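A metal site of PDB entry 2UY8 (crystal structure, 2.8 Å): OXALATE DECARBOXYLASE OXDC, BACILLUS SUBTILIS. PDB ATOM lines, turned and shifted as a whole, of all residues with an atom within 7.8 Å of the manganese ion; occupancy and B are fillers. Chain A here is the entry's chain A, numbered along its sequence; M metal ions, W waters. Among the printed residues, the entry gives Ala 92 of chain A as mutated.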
ATOM      1  N   MET A  84      -8.062   3.129  14.837  1.00  0.00           N
ATOM      2  CA  MET A  84      -7.042   4.156  14.803  1.00  0.00           C
ATOM      3  C   MET A  84      -7.389   5.348  13.887  1.00  0.00           C
ATOM      4  O   MET A  84      -7.872   5.172  12.748  1.00  0.00           O
ATOM      5  CB  MET A  84      -5.690   3.568  14.420  1.00  0.00           C
ATOM      6  CG  MET A  84      -4.610   4.598  14.284  1.00  0.00           C
ATOM      7  SD  MET A  84      -2.895   4.022  14.159  1.00  0.00           S
ATOM      8  CE  MET A  84      -2.555   3.395  15.811  1.00  0.00           C
ATOM      9  N   ALA A  92       1.811   7.147  12.060  1.00  0.00           N
ATOM     10  CA  ALA A  92       1.854   5.982  12.958  1.00  0.00           C
ATOM     11  C   ALA A  92       3.279   5.545  12.800  1.00  0.00           C
ATOM     12  O   ALA A  92       3.698   5.123  11.715  1.00  0.00           O
ATOM     13  CB  ALA A  92       0.894   4.894  12.538  1.00  0.00           C
ATOM     14  N   GLU A  93       4.056   5.768  13.851  1.00  0.00           N
ATOM     15  CA  GLU A  93       5.513   5.646  13.801  1.00  0.00           C
ATOM     16  C   GLU A  93       5.926   4.263  13.249  1.00  0.00           C
ATOM     17  O   GLU A  93       5.371   3.219  13.650  1.00  0.00           O
ATOM     18  CB  GLU A  93       6.078   5.894  15.193  1.00  0.00           C
ATOM     19  CG  GLU A  93       7.500   5.490  15.306  1.00  0.00           C
ATOM     20  CD  GLU A  93       8.032   5.437  16.741  1.00  0.00           C
ATOM     21  OE1 GLU A  93       7.262   5.540  17.740  1.00  0.00           O
ATOM     22  OE2 GLU A  93       9.261   5.276  16.830  1.00  0.00           O
ATOM     23  N   LEU A  94       6.878   4.278  12.321  1.00  0.00           N
ATOM     24  CA  LEU A  94       7.513   3.058  11.844  1.00  0.00           C
ATOM     25  C   LEU A  94       7.660   2.010  12.933  1.00  0.00           C
ATOM     26  O   LEU A  94       8.259   2.261  13.985  1.00  0.00           O
ATOM     27  CB  LEU A  94       8.895   3.395  11.330  1.00  0.00           C
ATOM     28  CG  LEU A  94       8.950   3.870   9.891  1.00  0.00           C
ATOM     29  CD1 LEU A  94      10.326   4.501   9.743  1.00  0.00           C
ATOM     30  CD2 LEU A  94       8.669   2.696   8.964  1.00  0.00           C
ATOM     31  N   HIS A  95       7.130   0.829  12.688  1.00  0.00           N
ATOM     32  CA  HIS A  95       7.091  -0.186  13.706  1.00  0.00           C
ATOM     33  C   HIS A  95       6.910  -1.558  13.090  1.00  0.00           C
ATOM     34  O   HIS A  95       6.750  -1.676  11.866  1.00  0.00           O
ATOM     35  CB  HIS A  95       5.955   0.151  14.674  1.00  0.00           C
ATOM     36  CG  HIS A  95       4.602   0.006  14.077  1.00  0.00           C
ATOM     37  ND1 HIS A  95       4.002   1.008  13.346  1.00  0.00           N
ATOM     38  CD2 HIS A  95       3.726  -1.023  14.113  1.00  0.00           C
ATOM     39  CE1 HIS A  95       2.802   0.598  12.960  1.00  0.00           C
ATOM     40  NE2 HIS A  95       2.602  -0.621  13.407  1.00  0.00           N
ATOM     41  N   TRP A  96       6.968  -2.592  13.941  1.00  0.00           N
ATOM     42  CA  TRP A  96       6.543  -3.948  13.550  1.00  0.00           C
ATOM     43  C   TRP A  96       5.797  -4.755  14.668  1.00  0.00           C
ATOM     44  O   TRP A  96       5.862  -4.385  15.853  1.00  0.00           O
ATOM     45  CB  TRP A  96       7.703  -4.714  12.945  1.00  0.00           C
ATOM     46  CG  TRP A  96       8.710  -5.232  13.934  1.00  0.00           C
ATOM     47  CD1 TRP A  96       8.741  -6.496  14.481  1.00  0.00           C
ATOM     48  CD2 TRP A  96       9.829  -4.535  14.483  1.00  0.00           C
ATOM     49  NE1 TRP A  96       9.818  -6.616  15.315  1.00  0.00           N
ATOM     50  CE2 TRP A  96      10.499  -5.433  15.340  1.00  0.00           C
ATOM     51  CE3 TRP A  96      10.329  -3.218  14.340  1.00  0.00           C
ATOM     52  CZ2 TRP A  96      11.653  -5.075  16.066  1.00  0.00           C
ATOM     53  CZ3 TRP A  96      11.494  -2.854  15.047  1.00  0.00           C
ATOM     54  CH2 TRP A  96      12.129  -3.790  15.912  1.00  0.00           C
ATOM     55  N   HIS A  97       5.089  -5.807  14.276  1.00  0.00           N
ATOM     56  CA  HIS A  97       4.255  -6.605  15.187  1.00  0.00           C
ATOM     57  C   HIS A  97       4.610  -8.100  15.180  1.00  0.00           C
ATOM     58  O   HIS A  97       5.113  -8.621  14.174  1.00  0.00           O
ATOM     59  CB  HIS A  97       2.793  -6.552  14.733  1.00  0.00           C
ATOM     60  CG  HIS A  97       2.248  -5.179  14.536  1.00  0.00           C
ATOM     61  ND1 HIS A  97       2.046  -4.300  15.578  1.00  0.00           N
ATOM     62  CD2 HIS A  97       1.812  -4.554  13.427  1.00  0.00           C
ATOM     63  CE1 HIS A  97       1.534  -3.169  15.106  1.00  0.00           C
ATOM     64  NE2 HIS A  97       1.392  -3.299  13.804  1.00  0.00           N
ATOM     65  N   GLU A  99       2.048 -10.150  15.410  1.00  0.00           N
ATOM     66  CA  GLU A  99       0.879 -10.510  14.600  1.00  0.00           C
ATOM     67  C   GLU A  99       0.917  -9.947  13.153  1.00  0.00           C
ATOM     68  O   GLU A  99       1.518  -8.901  12.911  1.00  0.00           O
ATOM     69  CB  GLU A  99      -0.342  -9.982  15.291  1.00  0.00           C
ATOM     70  CG  GLU A  99      -0.483 -10.521  16.680  1.00  0.00           C
ATOM     71  CD  GLU A  99       0.322  -9.779  17.775  1.00  0.00           C
ATOM     72  OE1 GLU A  99       1.012  -8.745  17.506  1.00  0.00           O
ATOM     73  OE2 GLU A  99       0.248 -10.257  18.927  1.00  0.00           O
ATOM     74  N   ALA A 100       0.264 -10.643  12.221  1.00  0.00           N
ATOM     75  CA  ALA A 100      -0.073 -10.037  10.936  1.00  0.00           C
ATOM     76  C   ALA A 100      -1.144  -8.947  11.170  1.00  0.00           C
ATOM     77  O   ALA A 100      -1.992  -9.074  12.090  1.00  0.00           O
ATOM     78  CB  ALA A 100      -0.547 -11.086   9.901  1.00  0.00           C
ATOM     79  N   GLU A 101      -1.075  -7.884  10.358  1.00  0.00           N
ATOM     80  CA  GLU A 101      -2.003  -6.761  10.440  1.00  0.00           C
ATOM     81  C   GLU A 101      -2.868  -6.620   9.161  1.00  0.00           C
ATOM     82  O   GLU A 101      -2.351  -6.648   8.047  1.00  0.00           O
ATOM     83  CB  GLU A 101      -1.253  -5.470  10.693  1.00  0.00           C
ATOM     84  CG  GLU A 101      -2.084  -4.234  10.480  1.00  0.00           C
ATOM     85  CD  GLU A 101      -1.331  -2.990  10.817  1.00  0.00           C
ATOM     86  OE1 GLU A 101      -0.498  -3.028  11.739  1.00  0.00           O
ATOM     87  OE2 GLU A 101      -1.545  -1.952  10.174  1.00  0.00           O
ATOM     88  N   TRP A 102      -4.178  -6.459   9.353  1.00  0.00           N
ATOM     89  CA  TRP A 102      -5.086  -6.305   8.260  1.00  0.00           C
ATOM     90  C   TRP A 102      -5.861  -5.022   8.488  1.00  0.00           C
ATOM     91  O   TRP A 102      -6.178  -4.668   9.614  1.00  0.00           O
ATOM     92  CB  TRP A 102      -6.040  -7.485   8.232  1.00  0.00           C
ATOM     93  CG  TRP A 102      -7.094  -7.436   7.122  1.00  0.00           C
ATOM     94  CD1 TRP A 102      -6.998  -8.026   5.864  1.00  0.00           C
ATOM     95  CD2 TRP A 102      -8.353  -6.774   7.160  1.00  0.00           C
ATOM     96  NE1 TRP A 102      -8.137  -7.780   5.145  1.00  0.00           N
ATOM     97  CE2 TRP A 102      -8.991  -7.015   5.909  1.00  0.00           C
ATOM     98  CE3 TRP A 102      -9.022  -6.008   8.115  1.00  0.00           C
ATOM     99  CZ2 TRP A 102     -10.274  -6.500   5.597  1.00  0.00           C
ATOM    100  CZ3 TRP A 102     -10.331  -5.476   7.798  1.00  0.00           C
ATOM    101  CH2 TRP A 102     -10.915  -5.737   6.557  1.00  0.00           C
ATOM    102  N   TRP A 132      -5.152  -2.971   3.428  1.00  0.00           N
ATOM    103  CA  TRP A 132      -3.773  -3.476   3.379  1.00  0.00           C
ATOM    104  C   TRP A 132      -3.636  -4.665   4.302  1.00  0.00           C
ATOM    105  O   TRP A 132      -4.456  -4.853   5.189  1.00  0.00           O
ATOM    106  CB  TRP A 132      -2.737  -2.393   3.729  1.00  0.00           C
ATOM    107  CG  TRP A 132      -2.744  -1.905   5.169  1.00  0.00           C
ATOM    108  CD1 TRP A 132      -2.328  -2.585   6.268  1.00  0.00           C
ATOM    109  CD2 TRP A 132      -3.164  -0.597   5.623  1.00  0.00           C
ATOM    110  NE1 TRP A 132      -2.479  -1.794   7.383  1.00  0.00           N
ATOM    111  CE2 TRP A 132      -2.992  -0.581   7.018  1.00  0.00           C
ATOM    112  CE3 TRP A 132      -3.687   0.536   4.998  1.00  0.00           C
ATOM    113  CZ2 TRP A 132      -3.312   0.543   7.793  1.00  0.00           C
ATOM    114  CZ3 TRP A 132      -3.993   1.629   5.757  1.00  0.00           C
ATOM    115  CH2 TRP A 132      -3.807   1.629   7.144  1.00  0.00           C
ATOM    116  N   PHE A 134      -0.229  -6.515   6.251  1.00  0.00           N
ATOM    117  CA  PHE A 134       1.207  -6.592   6.540  1.00  0.00           C
ATOM    118  C   PHE A 134       1.558  -7.893   7.271  1.00  0.00           C
ATOM    119  O   PHE A 134       1.187  -8.071   8.460  1.00  0.00           O
ATOM    120  CB  PHE A 134       1.617  -5.413   7.436  1.00  0.00           C
ATOM    121  CG  PHE A 134       1.307  -4.040   6.860  1.00  0.00           C
ATOM    122  CD1 PHE A 134       1.373  -3.792   5.466  1.00  0.00           C
ATOM    123  CD2 PHE A 134       0.995  -2.970   7.731  1.00  0.00           C
ATOM    124  CE1 PHE A 134       1.094  -2.497   4.960  1.00  0.00           C
ATOM    125  CE2 PHE A 134       0.733  -1.698   7.239  1.00  0.00           C
ATOM    126  CZ  PHE A 134       0.771  -1.462   5.832  1.00  0.00           C
ATOM    127  N   LEU A 138       7.091  -7.862   9.520  1.00  0.00           N
ATOM    128  CA  LEU A 138       7.591  -6.943   8.529  1.00  0.00           C
ATOM    129  C   LEU A 138       7.260  -5.527   8.910  1.00  0.00           C
ATOM    130  O   LEU A 138       6.118  -5.244   9.253  1.00  0.00           O
ATOM    131  CB  LEU A 138       7.010  -7.238   7.158  1.00  0.00           C
ATOM    132  CG  LEU A 138       7.356  -8.599   6.584  1.00  0.00           C
ATOM    133  CD1 LEU A 138       6.658  -8.722   5.256  1.00  0.00           C
ATOM    134  CD2 LEU A 138       8.858  -8.815   6.466  1.00  0.00           C
ATOM    135  N   PRO A 139       8.243  -4.612   8.847  1.00  0.00           N
ATOM    136  CA  PRO A 139       8.067  -3.265   9.378  1.00  0.00           C
ATOM    137  C   PRO A 139       7.295  -2.388   8.424  1.00  0.00           C
ATOM    138  O   PRO A 139       7.397  -2.529   7.212  1.00  0.00           O
ATOM    139  CB  PRO A 139       9.490  -2.743   9.487  1.00  0.00           C
ATOM    140  CG  PRO A 139      10.252  -3.493   8.505  1.00  0.00           C
ATOM    141  CD  PRO A 139       9.567  -4.799   8.243  1.00  0.00           C
ATOM    142  N   HIS A 140       6.526  -1.477   8.990  1.00  0.00           N
ATOM    143  CA  HIS A 140       5.619  -0.706   8.174  1.00  0.00           C
ATOM    144  C   HIS A 140       5.349   0.628   8.833  1.00  0.00           C
ATOM    145  O   HIS A 140       5.726   0.868  10.003  1.00  0.00           O
ATOM    146  CB  HIS A 140       4.325  -1.498   7.929  1.00  0.00           C
ATOM    147  CG  HIS A 140       3.612  -1.948   9.173  1.00  0.00           C
ATOM    148  ND1 HIS A 140       3.767  -3.219   9.708  1.00  0.00           N
ATOM    149  CD2 HIS A 140       2.722  -1.319   9.980  1.00  0.00           C
ATOM    150  CE1 HIS A 140       3.024  -3.337  10.786  1.00  0.00           C
ATOM    151  NE2 HIS A 140       2.382  -2.199  10.983  1.00  0.00           N
ATOM    152  N   SER A 141       4.681   1.495   8.079  1.00  0.00           N
ATOM    153  CA  SER A 141       4.165   2.727   8.676  1.00  0.00           C
ATOM    154  C   SER A 141       2.888   3.154   7.995  1.00  0.00           C
ATOM    155  O   SER A 141       2.556   2.676   6.877  1.00  0.00           O
ATOM    156  CB  SER A 141       5.185   3.872   8.584  1.00  0.00           C
ATOM    157  OG  SER A 141       5.431   4.243   7.232  1.00  0.00           O
ATOM    158  N   ILE A 142       2.173   4.064   8.671  1.00  0.00           N
ATOM    159  CA  ILE A 142       0.983   4.701   8.133  1.00  0.00           C
ATOM    160  C   ILE A 142       1.162   6.213   8.324  1.00  0.00           C
ATOM    161  O   ILE A 142       1.532   6.663   9.410  1.00  0.00           O
ATOM    162  CB  ILE A 142      -0.320   4.206   8.852  1.00  0.00           C
ATOM    163  CG1 ILE A 142      -0.388   2.695   8.820  1.00  0.00           C
ATOM    164  CG2 ILE A 142      -1.647   4.814   8.254  1.00  0.00           C
ATOM    165  CD1 ILE A 142      -0.996   2.153  10.025  1.00  0.00           C
ATOM    166  N   PHE A 151      -9.408   4.277  10.372  1.00  0.00           N
ATOM    167  CA  PHE A 151      -9.417   2.923   9.822  1.00  0.00           C
ATOM    168  C   PHE A 151      -9.441   1.890  10.955  1.00  0.00           C
ATOM    169  O   PHE A 151      -9.147   2.202  12.108  1.00  0.00           O
ATOM    170  CB  PHE A 151      -8.192   2.707   8.921  1.00  0.00           C
ATOM    171  CG  PHE A 151      -6.924   3.161   9.538  1.00  0.00           C
ATOM    172  CD1 PHE A 151      -6.504   4.482   9.403  1.00  0.00           C
ATOM    173  CD2 PHE A 151      -6.190   2.289  10.333  1.00  0.00           C
ATOM    174  CE1 PHE A 151      -5.347   4.914  10.024  1.00  0.00           C
ATOM    175  CE2 PHE A 151      -5.021   2.720  10.966  1.00  0.00           C
ATOM    176  CZ  PHE A 151      -4.600   4.040  10.821  1.00  0.00           C
ATOM    177  N   LEU A 153      -8.066  -1.766  12.249  1.00  0.00           N
ATOM    178  CA  LEU A 153      -6.964  -2.693  12.070  1.00  0.00           C
ATOM    179  C   LEU A 153      -7.367  -4.003  12.684  1.00  0.00           C
ATOM    180  O   LEU A 153      -8.015  -4.012  13.739  1.00  0.00           O
ATOM    181  CB  LEU A 153      -5.708  -2.199  12.744  1.00  0.00           C
ATOM    182  CG  LEU A 153      -5.049  -0.897  12.323  1.00  0.00           C
ATOM    183  CD1 LEU A 153      -3.943  -0.594  13.308  1.00  0.00           C
ATOM    184  CD2 LEU A 153      -4.495  -0.914  10.899  1.00  0.00           C
ATOM    185  N   PHE A 155      -5.650  -7.654  14.011  1.00  0.00           N
ATOM    186  CA  PHE A 155      -4.469  -8.466  14.263  1.00  0.00           C
ATOM    187  C   PHE A 155      -4.868  -9.917  14.582  1.00  0.00           C
ATOM    188  O   PHE A 155      -5.849 -10.171  15.306  1.00  0.00           O
ATOM    189  CB  PHE A 155      -3.657  -7.865  15.398  1.00  0.00           C
ATOM    190  CG  PHE A 155      -3.231  -6.458  15.148  1.00  0.00           C
ATOM    191  CD1 PHE A 155      -4.010  -5.393  15.612  1.00  0.00           C
ATOM    192  CD2 PHE A 155      -2.058  -6.175  14.462  1.00  0.00           C
ATOM    193  CE1 PHE A 155      -3.617  -4.059  15.380  1.00  0.00           C
ATOM    194  CE2 PHE A 155      -1.649  -4.857  14.214  1.00  0.00           C
ATOM    195  CZ  PHE A 155      -2.427  -3.793  14.668  1.00  0.00           C
ATOM    196  N   PHE A 160      -3.243  -9.459  21.438  1.00  0.00           N
ATOM    197  CA  PHE A 160      -2.600  -8.210  21.078  1.00  0.00           C
ATOM    198  C   PHE A 160      -2.594  -7.207  22.256  1.00  0.00           C
ATOM    199  O   PHE A 160      -3.594  -7.004  22.960  1.00  0.00           O
ATOM    200  CB  PHE A 160      -3.298  -7.644  19.861  1.00  0.00           C
ATOM    201  CG  PHE A 160      -2.663  -6.388  19.287  1.00  0.00           C
ATOM    202  CD1 PHE A 160      -1.610  -6.471  18.382  1.00  0.00           C
ATOM    203  CD2 PHE A 160      -3.171  -5.127  19.589  1.00  0.00           C
ATOM    204  CE1 PHE A 160      -1.054  -5.312  17.831  1.00  0.00           C
ATOM    205  CE2 PHE A 160      -2.606  -3.947  19.039  1.00  0.00           C
ATOM    206  CZ  PHE A 160      -1.561  -4.041  18.173  1.00  0.00           C
ATOM    207  N   THR A 165       3.954  -4.932  19.816  1.00  0.00           N
ATOM    208  CA  THR A 165       4.483  -3.860  18.973  1.00  0.00           C
ATOM    209  C   THR A 165       5.871  -3.359  19.331  1.00  0.00           C
ATOM    210  O   THR A 165       6.182  -3.084  20.489  1.00  0.00           O
ATOM    211  CB  THR A 165       3.524  -2.684  18.844  1.00  0.00           C
ATOM    212  OG1 THR A 165       2.285  -3.173  18.336  1.00  0.00           O
ATOM    213  CG2 THR A 165       4.034  -1.701  17.882  1.00  0.00           C
HETATM  214 MN    MN M   1       0.890  -1.794  12.592  1.00  0.00          MN
HETATM  215  O   HOH W   1      -0.567  -0.791  14.302  1.00  0.00           O
HETATM  216  O   HOH W   2       0.009  -0.230  11.581  1.00  0.00           O
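ND1 of His 97 lies within hydrogen-bond range of OG1 of Thr 165 (3.0 Å). The backbone carbonyl oxygen (O) of Glu 101 lies within hydrogen-bond range of the backbone NH (N) of Phe 134 (2.8 Å). The indole nitrogen (NE1) of Trp 132 lies within hydrogen-bond range of the side-chain carboxylate (OE2) of Glu 101. A ring nitrogen (ND1) of His 95 sits at hydrogen-bond distance from the backbone carbonyl oxygen (O) of Glu 93, at 2.6 Å. ND1 of His 140 sits at hydrogen-bond distance from O of Leu 138.
Of the 23 residues printed, 4 come within 4 Å of the manganese ion.
The manganese ion is bound by NE2 of His 97, 2.0 Å away. The manganese ion is bound by the side-chain carboxylate (OE1) of Glu 101 (2.0 Å). The manganese ion is bound by water W2 (2.1 Å). The manganese ion is bound by NE2 of His 95 (2.2 Å). NE2 of His 140 is bound to the manganese ion (2.2 Å). Water W1 is bound to the manganese ion. The manganese ion has six donor atoms within binding distance.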
